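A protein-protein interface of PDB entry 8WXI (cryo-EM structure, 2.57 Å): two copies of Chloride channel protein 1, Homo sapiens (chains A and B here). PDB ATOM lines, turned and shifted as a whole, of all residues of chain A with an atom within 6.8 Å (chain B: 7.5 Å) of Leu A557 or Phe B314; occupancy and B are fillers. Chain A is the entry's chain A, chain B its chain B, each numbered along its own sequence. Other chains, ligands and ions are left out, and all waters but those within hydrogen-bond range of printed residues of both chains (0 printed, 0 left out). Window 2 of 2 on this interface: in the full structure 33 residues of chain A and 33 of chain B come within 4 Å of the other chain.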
ATOM      1  N   PHE A 343     -12.669   9.909 -10.997  1.00  0.00           N
ATOM      2  CA  PHE A 343     -12.779   8.587 -10.336  1.00  0.00           C
ATOM      3  C   PHE A 343     -11.517   8.139  -9.590  1.00  0.00           C
ATOM      4  O   PHE A 343     -10.419   8.142 -10.139  1.00  0.00           O
ATOM      5  CB  PHE A 343     -13.325   7.468 -11.256  1.00  0.00           C
ATOM      6  CG  PHE A 343     -13.156   6.080 -10.692  1.00  0.00           C
ATOM      7  CD1 PHE A 343     -13.905   5.661  -9.600  1.00  0.00           C
ATOM      8  CD2 PHE A 343     -12.243   5.195 -11.246  1.00  0.00           C
ATOM      9  CE1 PHE A 343     -13.735   4.401  -9.066  1.00  0.00           C
ATOM     10  CE2 PHE A 343     -12.076   3.929 -10.720  1.00  0.00           C
ATOM     11  CZ  PHE A 343     -12.820   3.531  -9.629  1.00  0.00           C
ATOM     12  N   LEU A 345      -9.003   5.861  -8.793  1.00  0.00           N
ATOM     13  CA  LEU A 345      -8.510   4.601  -9.331  1.00  0.00           C
ATOM     14  C   LEU A 345      -7.962   3.671  -8.262  1.00  0.00           C
ATOM     15  O   LEU A 345      -7.593   2.546  -8.564  1.00  0.00           O
ATOM     16  CB  LEU A 345      -7.432   4.850 -10.383  1.00  0.00           C
ATOM     17  CG  LEU A 345      -7.793   4.821 -11.869  1.00  0.00           C
ATOM     18  CD1 LEU A 345      -8.553   3.559 -12.238  1.00  0.00           C
ATOM     19  CD2 LEU A 345      -8.550   6.067 -12.303  1.00  0.00           C
ATOM     20  N   LEU A 348     -10.626   1.175  -7.652  1.00  0.00           N
ATOM     21  CA  LEU A 348     -10.721   0.152  -8.695  1.00  0.00           C
ATOM     22  C   LEU A 348     -10.338  -1.261  -8.238  1.00  0.00           C
ATOM     23  O   LEU A 348     -11.005  -2.207  -8.615  1.00  0.00           O
ATOM     24  CB  LEU A 348      -9.966   0.569  -9.968  1.00  0.00           C
ATOM     25  CG  LEU A 348     -10.524   0.221 -11.350  1.00  0.00           C
ATOM     26  CD1 LEU A 348      -9.676  -0.844 -12.024  1.00  0.00           C
ATOM     27  CD2 LEU A 348     -11.985  -0.197 -11.311  1.00  0.00           C
ATOM     28  N   PHE A 351     -13.408  -2.682  -6.665  1.00  0.00           N
ATOM     29  CA  PHE A 351     -14.466  -2.959  -7.621  1.00  0.00           C
ATOM     30  C   PHE A 351     -14.113  -4.191  -8.424  1.00  0.00           C
ATOM     31  O   PHE A 351     -14.988  -4.952  -8.815  1.00  0.00           O
ATOM     32  CB  PHE A 351     -14.654  -1.773  -8.550  1.00  0.00           C
ATOM     33  CG  PHE A 351     -15.334  -0.611  -7.908  1.00  0.00           C
ATOM     34  CD1 PHE A 351     -16.601  -0.742  -7.392  1.00  0.00           C
ATOM     35  CD2 PHE A 351     -14.706   0.610  -7.819  1.00  0.00           C
ATOM     36  CE1 PHE A 351     -17.236   0.333  -6.811  1.00  0.00           C
ATOM     37  CE2 PHE A 351     -15.331   1.683  -7.225  1.00  0.00           C
ATOM     38  CZ  PHE A 351     -16.601   1.548  -6.728  1.00  0.00           C
ATOM     39  N   ILE A 527     -22.521  -1.689  -8.589  1.00  0.00           N
ATOM     40  CA  ILE A 527     -21.548  -2.534  -9.269  1.00  0.00           C
ATOM     41  C   ILE A 527     -21.771  -3.989  -8.922  1.00  0.00           C
ATOM     42  O   ILE A 527     -21.832  -4.832  -9.806  1.00  0.00           O
ATOM     43  CB  ILE A 527     -20.117  -2.147  -8.887  1.00  0.00           C
ATOM     44  CG1 ILE A 527     -19.975  -0.640  -8.871  1.00  0.00           C
ATOM     45  CG2 ILE A 527     -19.116  -2.717  -9.861  1.00  0.00           C
ATOM     46  CD1 ILE A 527     -19.157  -0.104 -10.006  1.00  0.00           C
ATOM     47  N   PHE A 547     -27.041   0.719 -15.149  1.00  0.00           N
ATOM     48  CA  PHE A 547     -26.880   2.133 -15.464  1.00  0.00           C
ATOM     49  C   PHE A 547     -28.210   2.814 -15.663  1.00  0.00           C
ATOM     50  O   PHE A 547     -28.464   3.857 -15.082  1.00  0.00           O
ATOM     51  CB  PHE A 547     -26.076   2.313 -16.741  1.00  0.00           C
ATOM     52  CG  PHE A 547     -24.622   2.013 -16.589  1.00  0.00           C
ATOM     53  CD1 PHE A 547     -23.958   2.303 -15.414  1.00  0.00           C
ATOM     54  CD2 PHE A 547     -23.915   1.450 -17.635  1.00  0.00           C
ATOM     55  CE1 PHE A 547     -22.615   2.032 -15.283  1.00  0.00           C
ATOM     56  CE2 PHE A 547     -22.577   1.164 -17.506  1.00  0.00           C
ATOM     57  CZ  PHE A 547     -21.929   1.451 -16.327  1.00  0.00           C
ATOM     58  N   ILE A 553     -24.378   6.962 -14.793  1.00  0.00           N
ATOM     59  CA  ILE A 553     -23.350   6.174 -15.467  1.00  0.00           C
ATOM     60  C   ILE A 553     -21.965   6.593 -15.016  1.00  0.00           C
ATOM     61  O   ILE A 553     -21.009   6.488 -15.776  1.00  0.00           O
ATOM     62  CB  ILE A 553     -23.412   6.367 -16.993  1.00  0.00           C
ATOM     63  CG1 ILE A 553     -23.666   7.835 -17.334  1.00  0.00           C
ATOM     64  CG2 ILE A 553     -24.494   5.501 -17.611  1.00  0.00           C
ATOM     65  CD1 ILE A 553     -22.904   8.317 -18.547  1.00  0.00           C
ATOM     66  N   ALA A 554     -21.845   7.073 -13.786  1.00  0.00           N
ATOM     67  CA  ALA A 554     -20.558   7.563 -13.299  1.00  0.00           C
ATOM     68  C   ALA A 554     -19.549   6.448 -13.109  1.00  0.00           C
ATOM     69  O   ALA A 554     -18.374   6.606 -13.431  1.00  0.00           O
ATOM     70  CB  ALA A 554     -20.750   8.324 -11.998  1.00  0.00           C
ATOM     71  N   HIS A 555     -20.000   5.323 -12.575  1.00  0.00           N
ATOM     72  CA  HIS A 555     -19.108   4.203 -12.337  1.00  0.00           C
ATOM     73  C   HIS A 555     -19.051   3.315 -13.560  1.00  0.00           C
ATOM     74  O   HIS A 555     -19.175   2.103 -13.439  1.00  0.00           O
ATOM     75  CB  HIS A 555     -19.617   3.382 -11.156  1.00  0.00           C
ATOM     76  CG  HIS A 555     -19.285   3.967  -9.820  1.00  0.00           C
ATOM     77  ND1 HIS A 555     -17.990   4.144  -9.386  1.00  0.00           N
ATOM     78  CD2 HIS A 555     -20.081   4.412  -8.819  1.00  0.00           C
ATOM     79  CE1 HIS A 555     -18.001   4.675  -8.176  1.00  0.00           C
ATOM     80  NE2 HIS A 555     -19.259   4.846  -7.810  1.00  0.00           N
ATOM     81  N   ILE A 556     -18.865   3.901 -14.738  1.00  0.00           N
ATOM     82  CA  ILE A 556     -18.887   3.100 -15.959  1.00  0.00           C
ATOM     83  C   ILE A 556     -17.712   2.138 -16.057  1.00  0.00           C
ATOM     84  O   ILE A 556     -17.913   0.936 -16.196  1.00  0.00           O
ATOM     85  CB  ILE A 556     -19.063   3.982 -17.225  1.00  0.00           C
ATOM     86  CG1 ILE A 556     -18.835   3.178 -18.505  1.00  0.00           C
ATOM     87  CG2 ILE A 556     -18.181   5.224 -17.165  1.00  0.00           C
ATOM     88  CD1 ILE A 556     -19.985   3.264 -19.482  1.00  0.00           C
ATOM     89  N   LEU A 557     -16.492   2.646 -15.956  1.00  0.00           N
ATOM     90  CA  LEU A 557     -15.324   1.779 -15.972  1.00  0.00           C
ATOM     91  C   LEU A 557     -15.309   0.787 -14.813  1.00  0.00           C
ATOM     92  O   LEU A 557     -15.142  -0.402 -15.049  1.00  0.00           O
ATOM     93  CB  LEU A 557     -14.021   2.590 -16.068  1.00  0.00           C
ATOM     94  CG  LEU A 557     -12.847   2.010 -16.860  1.00  0.00           C
ATOM     95  CD1 LEU A 557     -11.787   1.450 -15.924  1.00  0.00           C
ATOM     96  CD2 LEU A 557     -13.301   0.967 -17.871  1.00  0.00           C
ATOM     97  N   PRO A 558     -15.485   1.251 -13.555  1.00  0.00           N
ATOM     98  CA  PRO A 558     -15.550   0.237 -12.500  1.00  0.00           C
ATOM     99  C   PRO A 558     -16.551  -0.888 -12.779  1.00  0.00           C
ATOM    100  O   PRO A 558     -16.208  -2.047 -12.563  1.00  0.00           O
ATOM    101  CB  PRO A 558     -16.004   1.045 -11.296  1.00  0.00           C
ATOM    102  CG  PRO A 558     -15.382   2.360 -11.495  1.00  0.00           C
ATOM    103  CD  PRO A 558     -15.472   2.607 -12.968  1.00  0.00           C
ATOM    104  N   MET A 559     -17.750  -0.562 -13.255  1.00  0.00           N
ATOM    105  CA  MET A 559     -18.751  -1.580 -13.523  1.00  0.00           C
ATOM    106  C   MET A 559     -18.323  -2.510 -14.630  1.00  0.00           C
ATOM    107  O   MET A 559     -18.387  -3.711 -14.472  1.00  0.00           O
ATOM    108  CB  MET A 559     -20.112  -0.980 -13.853  1.00  0.00           C
ATOM    109  CG  MET A 559     -21.272  -1.884 -13.472  1.00  0.00           C
ATOM    110  SD  MET A 559     -22.833  -1.020 -13.248  1.00  0.00           S
ATOM    111  CE  MET A 559     -22.351   0.261 -12.096  1.00  0.00           C
ATOM    112  N   MET A 560     -17.879  -1.960 -15.746  1.00  0.00           N
ATOM    113  CA  MET A 560     -17.437  -2.774 -16.859  1.00  0.00           C
ATOM    114  C   MET A 560     -16.407  -3.778 -16.408  1.00  0.00           C
ATOM    115  O   MET A 560     -16.572  -4.964 -16.639  1.00  0.00           O
ATOM    116  CB  MET A 560     -16.862  -1.897 -17.959  1.00  0.00           C
ATOM    117  CG  MET A 560     -17.563  -2.049 -19.292  1.00  0.00           C
ATOM    118  SD  MET A 560     -18.519  -0.586 -19.718  1.00  0.00           S
ATOM    119  CE  MET A 560     -20.180  -1.148 -19.360  1.00  0.00           C
ATOM    120  N   VAL A 561     -15.355  -3.312 -15.750  1.00  0.00           N
ATOM    121  CA  VAL A 561     -14.325  -4.203 -15.240  1.00  0.00           C
ATOM    122  C   VAL A 561     -14.942  -5.305 -14.397  1.00  0.00           C
ATOM    123  O   VAL A 561     -14.734  -6.475 -14.672  1.00  0.00           O
ATOM    124  CB  VAL A 561     -13.275  -3.417 -14.426  1.00  0.00           C
ATOM    125  CG1 VAL A 561     -12.339  -4.344 -13.667  1.00  0.00           C
ATOM    126  CG2 VAL A 561     -12.478  -2.509 -15.346  1.00  0.00           C
ATOM    127  N   ALA A 562     -15.732  -4.937 -13.398  1.00  0.00           N
ATOM    128  CA  ALA A 562     -16.349  -5.919 -12.521  1.00  0.00           C
ATOM    129  C   ALA A 562     -17.184  -6.961 -13.236  1.00  0.00           C
ATOM    130  O   ALA A 562     -17.026  -8.137 -12.987  1.00  0.00           O
ATOM    131  CB  ALA A 562     -17.186  -5.221 -11.477  1.00  0.00           C
ATOM    132  N   GLY B 125      -6.662  -3.480 -26.797  1.00  0.00           N
ATOM    133  CA  GLY B 125      -7.004  -2.364 -25.941  1.00  0.00           C
ATOM    134  C   GLY B 125      -5.827  -1.506 -25.566  1.00  0.00           C
ATOM    135  O   GLY B 125      -5.879  -0.295 -25.716  1.00  0.00           O
ATOM    136  N   LEU B 126      -4.756  -2.127 -25.095  1.00  0.00           N
ATOM    137  CA  LEU B 126      -3.565  -1.389 -24.707  1.00  0.00           C
ATOM    138  C   LEU B 126      -3.023  -0.557 -25.845  1.00  0.00           C
ATOM    139  O   LEU B 126      -2.882   0.649 -25.709  1.00  0.00           O
ATOM    140  CB  LEU B 126      -2.486  -2.352 -24.216  1.00  0.00           C
ATOM    141  CG  LEU B 126      -1.107  -1.792 -23.888  1.00  0.00           C
ATOM    142  CD1 LEU B 126      -1.064  -1.270 -22.464  1.00  0.00           C
ATOM    143  CD2 LEU B 126      -0.053  -2.863 -24.110  1.00  0.00           C
ATOM    144  N   ALA B 129      -5.407   2.306 -27.079  1.00  0.00           N
ATOM    145  CA  ALA B 129      -5.467   3.426 -26.167  1.00  0.00           C
ATOM    146  C   ALA B 129      -4.201   4.232 -26.242  1.00  0.00           C
ATOM    147  O   ALA B 129      -4.253   5.443 -26.217  1.00  0.00           O
ATOM    148  CB  ALA B 129      -5.691   2.948 -24.757  1.00  0.00           C
ATOM    149  N   PRO B 282     -16.578   2.620 -24.275  1.00  0.00           N
ATOM    150  CA  PRO B 282     -16.527   1.160 -24.396  1.00  0.00           C
ATOM    151  C   PRO B 282     -17.827   0.586 -24.960  1.00  0.00           C
ATOM    152  O   PRO B 282     -17.807   0.118 -26.084  1.00  0.00           O
ATOM    153  CB  PRO B 282     -16.333   0.703 -22.955  1.00  0.00           C
ATOM    154  CG  PRO B 282     -15.667   1.850 -22.282  1.00  0.00           C
ATOM    155  CD  PRO B 282     -16.218   3.086 -22.927  1.00  0.00           C
ATOM    156  N   ALA B 308     -12.052  -5.941 -24.778  1.00  0.00           N
ATOM    157  CA  ALA B 308     -10.959  -5.166 -25.328  1.00  0.00           C
ATOM    158  C   ALA B 308     -11.182  -3.666 -25.208  1.00  0.00           C
ATOM    159  O   ALA B 308     -10.239  -2.919 -24.981  1.00  0.00           O
ATOM    160  CB  ALA B 308     -10.716  -5.572 -26.760  1.00  0.00           C
ATOM    161  N   ALA B 309     -12.428  -3.220 -25.335  1.00  0.00           N
ATOM    162  CA  ALA B 309     -12.738  -1.802 -25.224  1.00  0.00           C
ATOM    163  C   ALA B 309     -12.665  -1.302 -23.792  1.00  0.00           C
ATOM    164  O   ALA B 309     -12.347  -0.144 -23.554  1.00  0.00           O
ATOM    165  CB  ALA B 309     -14.103  -1.508 -25.810  1.00  0.00           C
ATOM    166  N   THR B 310     -12.960  -2.168 -22.832  1.00  0.00           N
ATOM    167  CA  THR B 310     -12.854  -1.769 -21.439  1.00  0.00           C
ATOM    168  C   THR B 310     -11.402  -1.743 -21.030  1.00  0.00           C
ATOM    169  O   THR B 310     -11.024  -0.983 -20.146  1.00  0.00           O
ATOM    170  CB  THR B 310     -13.664  -2.676 -20.498  1.00  0.00           C
ATOM    171  OG1 THR B 310     -13.330  -4.045 -20.736  1.00  0.00           O
ATOM    172  CG2 THR B 310     -15.153  -2.474 -20.720  1.00  0.00           C
ATOM    173  N   PHE B 311     -10.572  -2.557 -21.672  1.00  0.00           N
ATOM    174  CA  PHE B 311      -9.148  -2.493 -21.386  1.00  0.00           C
ATOM    175  C   PHE B 311      -8.628  -1.184 -21.929  1.00  0.00           C
ATOM    176  O   PHE B 311      -7.844  -0.514 -21.273  1.00  0.00           O
ATOM    177  CB  PHE B 311      -8.388  -3.660 -22.002  1.00  0.00           C
ATOM    178  CG  PHE B 311      -7.059  -3.898 -21.365  1.00  0.00           C
ATOM    179  CD1 PHE B 311      -6.975  -4.510 -20.131  1.00  0.00           C
ATOM    180  CD2 PHE B 311      -5.897  -3.481 -21.981  1.00  0.00           C
ATOM    181  CE1 PHE B 311      -5.754  -4.722 -19.530  1.00  0.00           C
ATOM    182  CE2 PHE B 311      -4.670  -3.686 -21.387  1.00  0.00           C
ATOM    183  CZ  PHE B 311      -4.597  -4.308 -20.158  1.00  0.00           C
ATOM    184  N   SER B 312      -9.077  -0.802 -23.118  1.00  0.00           N
ATOM    185  CA  SER B 312      -8.685   0.474 -23.691  1.00  0.00           C
ATOM    186  C   SER B 312      -9.045   1.605 -22.749  1.00  0.00           C
ATOM    187  O   SER B 312      -8.237   2.488 -22.506  1.00  0.00           O
ATOM    188  CB  SER B 312      -9.387   0.674 -25.029  1.00  0.00           C
ATOM    189  OG  SER B 312      -8.461   0.922 -26.068  1.00  0.00           O
ATOM    190  N   ALA B 313     -10.254   1.574 -22.202  1.00  0.00           N
ATOM    191  CA  ALA B 313     -10.697   2.608 -21.277  1.00  0.00           C
ATOM    192  C   ALA B 313      -9.868   2.667 -20.011  1.00  0.00           C
ATOM    193  O   ALA B 313      -9.608   3.745 -19.491  1.00  0.00           O
ATOM    194  CB  ALA B 313     -12.154   2.391 -20.931  1.00  0.00           C
ATOM    195  N   PHE B 314      -9.460   1.516 -19.503  1.00  0.00           N
ATOM    196  CA  PHE B 314      -8.642   1.476 -18.300  1.00  0.00           C
ATOM    197  C   PHE B 314      -7.271   2.082 -18.576  1.00  0.00           C
ATOM    198  O   PHE B 314      -6.765   2.864 -17.775  1.00  0.00           O
ATOM    199  CB  PHE B 314      -8.568   0.034 -17.761  1.00  0.00           C
ATOM    200  CG  PHE B 314      -7.233  -0.359 -17.191  1.00  0.00           C
ATOM    201  CD1 PHE B 314      -6.864   0.028 -15.912  1.00  0.00           C
ATOM    202  CD2 PHE B 314      -6.366  -1.156 -17.919  1.00  0.00           C
ATOM    203  CE1 PHE B 314      -5.642  -0.338 -15.390  1.00  0.00           C
ATOM    204  CE2 PHE B 314      -5.141  -1.523 -17.404  1.00  0.00           C
ATOM    205  CZ  PHE B 314      -4.780  -1.118 -16.136  1.00  0.00           C
ATOM    206  N   VAL B 315      -6.677   1.744 -19.717  1.00  0.00           N
ATOM    207  CA  VAL B 315      -5.374   2.284 -20.060  1.00  0.00           C
ATOM    208  C   VAL B 315      -5.512   3.785 -20.230  1.00  0.00           C
ATOM    209  O   VAL B 315      -4.684   4.544 -19.753  1.00  0.00           O
ATOM    210  CB  VAL B 315      -4.784   1.611 -21.316  1.00  0.00           C
ATOM    211  CG1 VAL B 315      -3.423   2.191 -21.667  1.00  0.00           C
ATOM    212  CG2 VAL B 315      -4.641   0.120 -21.092  1.00  0.00           C
ATOM    213  N   PHE B 316      -6.593   4.218 -20.865  1.00  0.00           N
ATOM    214  CA  PHE B 316      -6.847   5.646 -21.045  1.00  0.00           C
ATOM    215  C   PHE B 316      -6.895   6.375 -19.718  1.00  0.00           C
ATOM    216  O   PHE B 316      -6.381   7.480 -19.607  1.00  0.00           O
ATOM    217  CB  PHE B 316      -8.179   5.831 -21.741  1.00  0.00           C
ATOM    218  CG  PHE B 316      -8.077   6.512 -23.059  1.00  0.00           C
ATOM    219  CD1 PHE B 316      -6.855   6.688 -23.666  1.00  0.00           C
ATOM    220  CD2 PHE B 316      -9.210   6.979 -23.689  1.00  0.00           C
ATOM    221  CE1 PHE B 316      -6.767   7.319 -24.884  1.00  0.00           C
ATOM    222  CE2 PHE B 316      -9.124   7.618 -24.904  1.00  0.00           C
ATOM    223  CZ  PHE B 316      -7.898   7.791 -25.502  1.00  0.00           C
ATOM    224  N   ARG B 317      -7.516   5.769 -18.715  1.00  0.00           N
ATOM    225  CA  ARG B 317      -7.644   6.387 -17.402  1.00  0.00           C
ATOM    226  C   ARG B 317      -6.304   6.545 -16.716  1.00  0.00           C
ATOM    227  O   ARG B 317      -6.037   7.588 -16.139  1.00  0.00           O
ATOM    228  CB  ARG B 317      -8.579   5.567 -16.520  1.00  0.00           C
ATOM    229  CG  ARG B 317      -9.887   6.265 -16.196  1.00  0.00           C
ATOM    230  CD  ARG B 317     -11.038   5.691 -17.005  1.00  0.00           C
ATOM    231  NE  ARG B 317     -10.998   6.126 -18.397  1.00  0.00           N
ATOM    232  CZ  ARG B 317     -12.069   6.271 -19.168  1.00  0.00           C
ATOM    233  NH1 ARG B 317     -11.934   6.671 -20.424  1.00  0.00           N
ATOM    234  NH2 ARG B 317     -13.276   6.015 -18.683  1.00  0.00           N
ATOM    235  N   VAL B 318      -5.462   5.518 -16.769  1.00  0.00           N
ATOM    236  CA  VAL B 318      -4.131   5.630 -16.179  1.00  0.00           C
ATOM    237  C   VAL B 318      -3.219   6.583 -16.951  1.00  0.00           C
ATOM    238  O   VAL B 318      -2.337   7.191 -16.362  1.00  0.00           O
ATOM    239  CB  VAL B 318      -3.472   4.260 -15.891  1.00  0.00           C
ATOM    240  CG1 VAL B 318      -4.441   3.361 -15.147  1.00  0.00           C
ATOM    241  CG2 VAL B 318      -2.969   3.584 -17.152  1.00  0.00           C
ATOM    242  N   LEU B 319      -3.453   6.757 -18.249  1.00  0.00           N
ATOM    243  CA  LEU B 319      -2.668   7.706 -19.025  1.00  0.00           C
ATOM    244  C   LEU B 319      -3.099   9.093 -18.619  1.00  0.00           C
ATOM    245  O   LEU B 319      -2.279  10.005 -18.528  1.00  0.00           O
ATOM    246  CB  LEU B 319      -2.910   7.503 -20.511  1.00  0.00           C
ATOM    247  CG  LEU B 319      -2.091   6.429 -21.213  1.00  0.00           C
ATOM    248  CD1 LEU B 319      -2.848   5.911 -22.424  1.00  0.00           C
ATOM    249  CD2 LEU B 319      -0.743   6.994 -21.622  1.00  0.00           C
ATOM    250  N   ALA B 320      -4.393   9.258 -18.369  1.00  0.00           N
ATOM    251  CA  ALA B 320      -4.917  10.551 -17.947  1.00  0.00           C
ATOM    252  C   ALA B 320      -4.616  10.786 -16.485  1.00  0.00           C
ATOM    253  O   ALA B 320      -5.120  11.732 -15.891  1.00  0.00           O
ATOM    254  CB  ALA B 320      -6.410  10.622 -18.195  1.00  0.00           C
ATOM    255  N   GLU B 548     -22.383   8.020 -22.676  1.00  0.00           N
ATOM    256  CA  GLU B 548     -21.101   7.806 -22.033  1.00  0.00           C
ATOM    257  C   GLU B 548     -20.160   8.988 -22.164  1.00  0.00           C
ATOM    258  O   GLU B 548     -19.448   9.304 -21.221  1.00  0.00           O
ATOM    259  CB  GLU B 548     -20.450   6.552 -22.592  1.00  0.00           C
ATOM    260  CG  GLU B 548     -20.842   5.282 -21.864  1.00  0.00           C
ATOM    261  CD  GLU B 548     -20.708   4.054 -22.734  1.00  0.00           C
ATOM    262  OE1 GLU B 548     -21.575   3.848 -23.607  1.00  0.00           O
ATOM    263  OE2 GLU B 548     -19.730   3.301 -22.554  1.00  0.00           O
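The backbone carbonyl oxygen (O) of Ala B313 lies within hydrogen-bond range of the guanidinium group (NE) of Arg B317.
Among the printed residues, merely in contact across the chains: Ile A553 with Glu B548, Ile A556 with Glu B548, Leu A557 with Thr B310, Leu A557 with Ala B313, Leu A557 with Phe B314 and Met A560 with Thr B310.
Leu A557 touches just these residues of chain B: Thr B310, Ala B313 and Phe B314. Phe B314 touches just one residue of chain A: Leu A557. Printed residues of chain A within 4 Å of Thr B310: Leu A557 (3.8 Å) and Met A560 (2.8 Å). Of the printed residues of chain A, Ala B313 touches Leu A557. Printed residues of chain B within 4 Å of Ile A556: Glu B548. Of the printed residues of chain A, Glu B548 touches Ile A553 (3.96 Å) and Ile A556 (3.1 Å). Val A561 touches none of the printed residues of chain B. The nearest residue of chain B that does not touch Leu A557 is Arg B317 (4.1 Å).
Printed residues of chain A that touch a printed residue of chain B: Ile A553, Ile A556, Leu A557 and Met A560.
No position is printed for both chains. Of the 6 pairs that touch across the chains among the printed residues, none has its exchanged pair printed and touching as well.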
